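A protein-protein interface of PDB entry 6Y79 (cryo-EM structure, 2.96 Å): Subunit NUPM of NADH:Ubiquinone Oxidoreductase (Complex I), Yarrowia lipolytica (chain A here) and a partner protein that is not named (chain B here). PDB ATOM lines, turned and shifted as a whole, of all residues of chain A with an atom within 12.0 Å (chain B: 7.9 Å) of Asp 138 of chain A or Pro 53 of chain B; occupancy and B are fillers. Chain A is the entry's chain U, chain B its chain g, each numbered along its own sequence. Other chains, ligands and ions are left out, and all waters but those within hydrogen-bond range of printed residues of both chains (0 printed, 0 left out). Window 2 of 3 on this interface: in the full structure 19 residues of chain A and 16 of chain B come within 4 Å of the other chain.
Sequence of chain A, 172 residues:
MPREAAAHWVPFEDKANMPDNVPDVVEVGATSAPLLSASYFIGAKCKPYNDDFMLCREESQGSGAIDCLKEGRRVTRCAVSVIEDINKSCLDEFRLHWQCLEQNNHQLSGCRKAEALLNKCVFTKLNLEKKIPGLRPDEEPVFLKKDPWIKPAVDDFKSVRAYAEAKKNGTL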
ATOM      1  N   ILE A 132     -23.202 -26.725  -9.325  1.00  0.00           N
ATOM      2  CA  ILE A 132     -24.534 -26.284  -9.714  1.00  0.00           C
ATOM      3  C   ILE A 132     -24.995 -27.172 -10.869  1.00  0.00           C
ATOM      4  O   ILE A 132     -24.378 -27.157 -11.943  1.00  0.00           O
ATOM      5  CB  ILE A 132     -24.557 -24.803 -10.109  1.00  0.00           C
ATOM      6  CG1 ILE A 132     -24.205 -23.932  -8.907  1.00  0.00           C
ATOM      7  CG2 ILE A 132     -25.920 -24.428 -10.635  1.00  0.00           C
ATOM      8  CD1 ILE A 132     -24.115 -22.471  -9.224  1.00  0.00           C
ATOM      9  N   GLY A 134     -27.813 -28.753 -13.800  1.00  0.00           N
ATOM     10  CA  GLY A 134     -28.555 -28.128 -14.873  1.00  0.00           C
ATOM     11  C   GLY A 134     -27.749 -27.176 -15.723  1.00  0.00           C
ATOM     12  O   GLY A 134     -28.310 -26.541 -16.621  1.00  0.00           O
ATOM     13  N   LEU A 135     -26.457 -27.070 -15.474  1.00  0.00           N
ATOM     14  CA  LEU A 135     -25.578 -26.123 -16.131  1.00  0.00           C
ATOM     15  C   LEU A 135     -24.814 -26.922 -17.171  1.00  0.00           C
ATOM     16  O   LEU A 135     -23.901 -27.682 -16.839  1.00  0.00           O
ATOM     17  CB  LEU A 135     -24.657 -25.477 -15.105  1.00  0.00           C
ATOM     18  CG  LEU A 135     -23.711 -24.339 -15.445  1.00  0.00           C
ATOM     19  CD1 LEU A 135     -24.493 -23.119 -15.801  1.00  0.00           C
ATOM     20  CD2 LEU A 135     -22.835 -24.065 -14.240  1.00  0.00           C
ATOM     21  N   ARG A 136     -25.214 -26.776 -18.427  1.00  0.00           N
ATOM     22  CA  ARG A 136     -24.502 -27.401 -19.529  1.00  0.00           C
ATOM     23  C   ARG A 136     -23.118 -26.783 -19.656  1.00  0.00           C
ATOM     24  O   ARG A 136     -22.880 -25.686 -19.149  1.00  0.00           O
ATOM     25  CB  ARG A 136     -25.300 -27.228 -20.822  1.00  0.00           C
ATOM     26  CG  ARG A 136     -25.463 -25.801 -21.311  1.00  0.00           C
ATOM     27  CD  ARG A 136     -26.388 -25.733 -22.520  1.00  0.00           C
ATOM     28  NE  ARG A 136     -26.775 -24.359 -22.819  1.00  0.00           N
ATOM     29  CZ  ARG A 136     -26.042 -23.519 -23.541  1.00  0.00           C
ATOM     30  NH1 ARG A 136     -24.882 -23.916 -24.047  1.00  0.00           N
ATOM     31  NH2 ARG A 136     -26.467 -22.284 -23.757  1.00  0.00           N
ATOM     32  N   PRO A 137     -22.174 -27.468 -20.304  1.00  0.00           N
ATOM     33  CA  PRO A 137     -20.921 -26.801 -20.667  1.00  0.00           C
ATOM     34  C   PRO A 137     -21.164 -25.677 -21.671  1.00  0.00           C
ATOM     35  O   PRO A 137     -22.281 -25.499 -22.203  1.00  0.00           O
ATOM     36  CB  PRO A 137     -20.090 -27.912 -21.291  1.00  0.00           C
ATOM     37  CG  PRO A 137     -21.094 -28.900 -21.773  1.00  0.00           C
ATOM     38  CD  PRO A 137     -22.140 -28.884 -20.709  1.00  0.00           C
ATOM     39  N   ASP A 138     -20.070 -24.905 -21.908  1.00  0.00           N
ATOM     40  CA  ASP A 138     -20.064 -23.560 -22.556  1.00  0.00           C
ATOM     41  C   ASP A 138     -20.694 -22.492 -21.616  1.00  0.00           C
ATOM     42  O   ASP A 138     -20.799 -21.307 -21.946  1.00  0.00           O
ATOM     43  CB  ASP A 138     -20.632 -23.670 -24.009  1.00  0.00           C
ATOM     44  CG  ASP A 138     -21.176 -22.385 -24.625  1.00  0.00           C
ATOM     45  OD1 ASP A 138     -22.347 -22.118 -24.321  1.00  0.00           O
ATOM     46  OD2 ASP A 138     -20.520 -21.715 -25.462  1.00  0.00           O
ATOM     47  N   GLU A 139     -20.912 -22.846 -20.336  1.00  0.00           N
ATOM     48  CA  GLU A 139     -21.481 -21.943 -19.328  1.00  0.00           C
ATOM     49  C   GLU A 139     -20.662 -21.991 -18.039  1.00  0.00           C
ATOM     50  O   GLU A 139     -20.614 -23.025 -17.363  1.00  0.00           O
ATOM     51  CB  GLU A 139     -22.932 -22.311 -19.057  1.00  0.00           C
ATOM     52  CG  GLU A 139     -23.865 -21.988 -20.211  1.00  0.00           C
ATOM     53  CD  GLU A 139     -25.299 -22.388 -19.953  1.00  0.00           C
ATOM     54  OE1 GLU A 139     -25.548 -23.084 -18.959  1.00  0.00           O
ATOM     55  OE2 GLU A 139     -26.177 -22.019 -20.758  1.00  0.00           O
ATOM     56  N   GLU A 140     -20.068 -20.855 -17.671  1.00  0.00           N
ATOM     57  CA  GLU A 140     -19.242 -20.804 -16.464  1.00  0.00           C
ATOM     58  C   GLU A 140     -20.125 -20.771 -15.217  1.00  0.00           C
ATOM     59  O   GLU A 140     -21.164 -20.101 -15.215  1.00  0.00           O
ATOM     60  CB  GLU A 140     -18.301 -19.588 -16.489  1.00  0.00           C
ATOM     61  CG  GLU A 140     -18.970 -18.233 -16.710  1.00  0.00           C
ATOM     62  CD  GLU A 140     -17.987 -17.079 -16.649  1.00  0.00           C
ATOM     63  OE1 GLU A 140     -16.790 -17.330 -16.410  1.00  0.00           O
ATOM     64  OE2 GLU A 140     -18.413 -15.921 -16.834  1.00  0.00           O
ATOM     65  N   PRO A 141     -19.778 -21.507 -14.162  1.00  0.00           N
ATOM     66  CA  PRO A 141     -20.510 -21.363 -12.896  1.00  0.00           C
ATOM     67  C   PRO A 141     -20.170 -20.038 -12.230  1.00  0.00           C
ATOM     68  O   PRO A 141     -19.043 -19.552 -12.332  1.00  0.00           O
ATOM     69  CB  PRO A 141     -20.035 -22.561 -12.065  1.00  0.00           C
ATOM     70  CG  PRO A 141     -18.794 -23.039 -12.724  1.00  0.00           C
ATOM     71  CD  PRO A 141     -18.860 -22.658 -14.159  1.00  0.00           C
ATOM     72  N   VAL A 142     -21.165 -19.454 -11.555  1.00  0.00           N
ATOM     73  CA  VAL A 142     -21.090 -18.070 -11.093  1.00  0.00           C
ATOM     74  C   VAL A 142     -20.046 -17.855  -9.996  1.00  0.00           C
ATOM     75  O   VAL A 142     -19.375 -16.817  -9.974  1.00  0.00           O
ATOM     76  CB  VAL A 142     -22.499 -17.611 -10.654  1.00  0.00           C
ATOM     77  CG1 VAL A 142     -23.090 -18.506  -9.557  1.00  0.00           C
ATOM     78  CG2 VAL A 142     -22.508 -16.136 -10.242  1.00  0.00           C
ATOM     79  N   LEU A 144     -17.188 -19.139  -9.699  1.00  0.00           N
ATOM     80  CA  LEU A 144     -15.857 -19.377 -10.226  1.00  0.00           C
ATOM     81  C   LEU A 144     -15.310 -18.204 -11.019  1.00  0.00           C
ATOM     82  O   LEU A 144     -14.105 -18.168 -11.285  1.00  0.00           O
ATOM     83  CB  LEU A 144     -15.849 -20.608 -11.144  1.00  0.00           C
ATOM     84  CG  LEU A 144     -15.645 -22.030 -10.620  1.00  0.00           C
ATOM     85  CD1 LEU A 144     -14.312 -22.149  -9.913  1.00  0.00           C
ATOM     86  CD2 LEU A 144     -16.763 -22.477  -9.728  1.00  0.00           C
ATOM     87  N   LYS A 145     -16.155 -17.261 -11.408  1.00  0.00           N
ATOM     88  CA  LYS A 145     -15.762 -16.272 -12.391  1.00  0.00           C
ATOM     89  C   LYS A 145     -14.912 -15.172 -11.773  1.00  0.00           C
ATOM     90  O   LYS A 145     -15.010 -14.864 -10.582  1.00  0.00           O
ATOM     91  CB  LYS A 145     -16.992 -15.671 -13.053  1.00  0.00           C
ATOM     92  CG  LYS A 145     -17.895 -14.885 -12.145  1.00  0.00           C
ATOM     93  CD  LYS A 145     -19.037 -14.373 -12.989  1.00  0.00           C
ATOM     94  CE  LYS A 145     -18.484 -13.398 -14.018  1.00  0.00           C
ATOM     95  NZ  LYS A 145     -19.452 -13.040 -15.093  1.00  0.00           N
ATOM     96  N   ARG B  47     -28.073 -13.651 -32.730  1.00  0.00           N
ATOM     97  CA  ARG B  47     -27.425 -13.711 -31.427  1.00  0.00           C
ATOM     98  C   ARG B  47     -27.310 -15.146 -30.929  1.00  0.00           C
ATOM     99  O   ARG B  47     -26.280 -15.532 -30.367  1.00  0.00           O
ATOM    100  CB  ARG B  47     -28.174 -12.859 -30.413  1.00  0.00           C
ATOM    101  CG  ARG B  47     -27.443 -12.811 -29.110  1.00  0.00           C
ATOM    102  CD  ARG B  47     -28.324 -12.562 -27.960  1.00  0.00           C
ATOM    103  NE  ARG B  47     -29.545 -13.360 -27.948  1.00  0.00           N
ATOM    104  CZ  ARG B  47     -29.663 -14.538 -27.351  1.00  0.00           C
ATOM    105  NH1 ARG B  47     -30.816 -15.180 -27.375  1.00  0.00           N
ATOM    106  NH2 ARG B  47     -28.628 -15.074 -26.731  1.00  0.00           N
ATOM    107  N   ARG B  48     -28.347 -15.957 -31.144  1.00  0.00           N
ATOM    108  CA  ARG B  48     -28.279 -17.357 -30.753  1.00  0.00           C
ATOM    109  C   ARG B  48     -27.288 -18.144 -31.594  1.00  0.00           C
ATOM    110  O   ARG B  48     -26.783 -19.172 -31.136  1.00  0.00           O
ATOM    111  CB  ARG B  48     -29.661 -17.994 -30.843  1.00  0.00           C
ATOM    112  CG  ARG B  48     -30.627 -17.441 -29.841  1.00  0.00           C
ATOM    113  CD  ARG B  48     -31.858 -18.299 -29.713  1.00  0.00           C
ATOM    114  NE  ARG B  48     -32.822 -17.694 -28.803  1.00  0.00           N
ATOM    115  CZ  ARG B  48     -33.916 -17.056 -29.193  1.00  0.00           C
ATOM    116  NH1 ARG B  48     -34.204 -16.956 -30.480  1.00  0.00           N
ATOM    117  NH2 ARG B  48     -34.734 -16.533 -28.290  1.00  0.00           N
ATOM    118  N   LYS B  49     -26.992 -17.678 -32.806  1.00  0.00           N
ATOM    119  CA  LYS B  49     -25.977 -18.324 -33.623  1.00  0.00           C
ATOM    120  C   LYS B  49     -24.562 -17.891 -33.253  1.00  0.00           C
ATOM    121  O   LYS B  49     -23.654 -18.727 -33.228  1.00  0.00           O
ATOM    122  CB  LYS B  49     -26.245 -18.025 -35.097  1.00  0.00           C
ATOM    123  CG  LYS B  49     -25.279 -18.684 -36.061  1.00  0.00           C
ATOM    124  CD  LYS B  49     -25.924 -18.926 -37.403  1.00  0.00           C
ATOM    125  CE  LYS B  49     -26.880 -20.095 -37.339  1.00  0.00           C
ATOM    126  NZ  LYS B  49     -27.268 -20.571 -38.693  1.00  0.00           N
ATOM    127  N   TYR B  50     -24.351 -16.611 -32.943  1.00  0.00           N
ATOM    128  CA  TYR B  50     -23.002 -16.070 -32.842  1.00  0.00           C
ATOM    129  C   TYR B  50     -22.586 -15.659 -31.439  1.00  0.00           C
ATOM    130  O   TYR B  50     -21.527 -16.084 -30.972  1.00  0.00           O
ATOM    131  CB  TYR B  50     -22.858 -14.881 -33.794  1.00  0.00           C
ATOM    132  CG  TYR B  50     -22.963 -15.313 -35.232  1.00  0.00           C
ATOM    133  CD1 TYR B  50     -21.945 -16.041 -35.827  1.00  0.00           C
ATOM    134  CD2 TYR B  50     -24.085 -15.016 -35.986  1.00  0.00           C
ATOM    135  CE1 TYR B  50     -22.039 -16.451 -37.136  1.00  0.00           C
ATOM    136  CE2 TYR B  50     -24.189 -15.421 -37.295  1.00  0.00           C
ATOM    137  CZ  TYR B  50     -23.166 -16.135 -37.865  1.00  0.00           C
ATOM    138  OH  TYR B  50     -23.278 -16.535 -39.174  1.00  0.00           O
ATOM    139  N   LEU B  51     -23.375 -14.832 -30.752  1.00  0.00           N
ATOM    140  CA  LEU B  51     -22.903 -14.256 -29.496  1.00  0.00           C
ATOM    141  C   LEU B  51     -22.907 -15.282 -28.372  1.00  0.00           C
ATOM    142  O   LEU B  51     -21.847 -15.638 -27.847  1.00  0.00           O
ATOM    143  CB  LEU B  51     -23.746 -13.037 -29.129  1.00  0.00           C
ATOM    144  CG  LEU B  51     -23.576 -11.878 -30.107  1.00  0.00           C
ATOM    145  CD1 LEU B  51     -24.464 -10.723 -29.736  1.00  0.00           C
ATOM    146  CD2 LEU B  51     -22.135 -11.436 -30.139  1.00  0.00           C
ATOM    147  N   TYR B  52     -24.087 -15.800 -28.022  1.00  0.00           N
ATOM    148  CA  TYR B  52     -24.174 -16.806 -26.977  1.00  0.00           C
ATOM    149  C   TYR B  52     -25.513 -17.510 -27.073  1.00  0.00           C
ATOM    150  O   TYR B  52     -26.525 -16.849 -27.340  1.00  0.00           O
ATOM    151  CB  TYR B  52     -23.983 -16.199 -25.578  1.00  0.00           C
ATOM    152  CG  TYR B  52     -24.883 -15.046 -25.222  1.00  0.00           C
ATOM    153  CD1 TYR B  52     -24.621 -13.747 -25.652  1.00  0.00           C
ATOM    154  CD2 TYR B  52     -25.967 -15.253 -24.415  1.00  0.00           C
ATOM    155  CE1 TYR B  52     -25.454 -12.707 -25.309  1.00  0.00           C
ATOM    156  CE2 TYR B  52     -26.779 -14.234 -24.066  1.00  0.00           C
ATOM    157  CZ  TYR B  52     -26.535 -12.967 -24.512  1.00  0.00           C
ATOM    158  OH  TYR B  52     -27.396 -11.980 -24.127  1.00  0.00           O
ATOM    159  N   PRO B  53     -25.562 -18.822 -26.886  1.00  0.00           N
ATOM    160  CA  PRO B  53     -26.844 -19.525 -26.836  1.00  0.00           C
ATOM    161  C   PRO B  53     -27.558 -19.273 -25.515  1.00  0.00           C
ATOM    162  O   PRO B  53     -27.024 -18.662 -24.590  1.00  0.00           O
ATOM    163  CB  PRO B  53     -26.458 -20.997 -26.988  1.00  0.00           C
ATOM    164  CG  PRO B  53     -25.040 -21.073 -26.606  1.00  0.00           C
ATOM    165  CD  PRO B  53     -24.415 -19.744 -26.859  1.00  0.00           C
ATOM    166  N   ASP B  54     -28.784 -19.778 -25.439  1.00  0.00           N
ATOM    167  CA  ASP B  54     -29.678 -19.415 -24.351  1.00  0.00           C
ATOM    168  C   ASP B  54     -29.304 -20.095 -23.039  1.00  0.00           C
ATOM    169  O   ASP B  54     -28.658 -21.146 -23.016  1.00  0.00           O
ATOM    170  CB  ASP B  54     -31.121 -19.757 -24.707  1.00  0.00           C
ATOM    171  CG  ASP B  54     -31.646 -18.945 -25.872  1.00  0.00           C
ATOM    172  OD1 ASP B  54     -31.270 -17.767 -26.007  1.00  0.00           O
ATOM    173  OD2 ASP B  54     -32.450 -19.497 -26.654  1.00  0.00           O
ATOM    174  N   HIS B  55     -29.725 -19.479 -21.939  1.00  0.00           N
ATOM    175  CA  HIS B  55     -29.467 -20.040 -20.628  1.00  0.00           C
ATOM    176  C   HIS B  55     -30.401 -21.215 -20.365  1.00  0.00           C
ATOM    177  O   HIS B  55     -31.465 -21.351 -20.971  1.00  0.00           O
ATOM    178  CB  HIS B  55     -29.617 -18.971 -19.545  1.00  0.00           C
ATOM    179  CG  HIS B  55     -31.015 -18.466 -19.368  1.00  0.00           C
ATOM    180  ND1 HIS B  55     -31.620 -17.621 -20.270  1.00  0.00           N
ATOM    181  CD2 HIS B  55     -31.916 -18.666 -18.379  1.00  0.00           C
ATOM    182  CE1 HIS B  55     -32.838 -17.335 -19.853  1.00  0.00           C
ATOM    183  NE2 HIS B  55     -33.043 -17.957 -18.708  1.00  0.00           N
ATOM    184  N   SER B  56     -29.977 -22.075 -19.466  1.00  0.00           N
ATOM    185  CA  SER B  56     -30.779 -23.213 -19.062  1.00  0.00           C
ATOM    186  C   SER B  56     -31.833 -22.767 -18.046  1.00  0.00           C
ATOM    187  O   SER B  56     -31.618 -21.796 -17.319  1.00  0.00           O
ATOM    188  CB  SER B  56     -29.876 -24.291 -18.475  1.00  0.00           C
ATOM    189  OG  SER B  56     -29.002 -24.794 -19.470  1.00  0.00           O
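Asp 138 of chain A touches one residue of chain B. Pro 53 of chain B touches just these residues of chain A: Arg 136 (3.4 Å) and Asp 138 (3.7 Å). No residue of chain A comes within 4 Å of Tyr 52 of chain B. Asp 54 of chain B touches just these residues of chain A: Arg 136 and Glu 139. Of the printed residues of chain A, His 55 of chain B touches Glu 139. Of the printed residues of chain B, Gly 134 of chain A touches Ser 56 (3.3 Å). The nearest residue of chain B that does not touch Asp 138 of chain A is Tyr 52 of chain B (6.2 Å). The nearest printed residue of chain B that does not touch Arg 136 of chain A is Ser 56 of chain B (4.05 Å).
Among the printed residues, merely in contact across the chains: Arg 136 of chain A with Pro 53 of chain B (3.4 Å), Asp 138 of chain A with Pro 53 of chain B (3.7 Å), Glu 139 of chain A with His 55 of chain B (3.8 Å) and Glu 139 of chain A with Ser 56 of chain B (3.9 Å).
The guanidinium group (NH2) of Arg 136 of chain A lies within hydrogen-bond range of the backbone carbonyl oxygen (O) of Asp 54 of chain B (2.6 Å). O of Asp 54 of chain B sits close to OE2 of Glu 139 of chain A (3.5 Å). The side-chain hydroxyl (OG) of Ser 56 of chain B sits close to the backbone carbonyl oxygen (O) of Gly 134 of chain A.
Printed residues of chain B that touch a printed residue of chain A: Pro 53, Asp 54, His 55 and Ser 56. Hydrophobic or aromatic side chains of chain B that line the printed part of chain A: Pro 53. Of the 12 printed residues of chain A, 4 touch a printed residue of chain B. Printed residues of chain A that touch a printed residue of chain B: Gly 134, Arg 136, Asp 138 and Glu 139. Among the printed residues, no Asp or Glu carboxylate lies within 4 Å of a Lys or Arg side-chain nitrogen of the other chain.
OD2 of Asp 54 of chain B is in salt-bridge range of NE of Arg 48 of chain B, at 2.8 Å. The guanidinium group (NH2) of Arg 136 of chain A is in salt-bridge range of the side-chain carboxylate (OE2) of Glu 139 of chain A, 3.0 Å away. The side-chain carboxylate of Asp 54 of chain B is in salt-bridge range of the guanidinium group of Arg 47 of chain B, at 3.0 Å. The side-chain carboxylate of Asp 138 of chain A lies within salt-bridge range of the guanidinium group of Arg 136 of chain A (3.1 Å).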
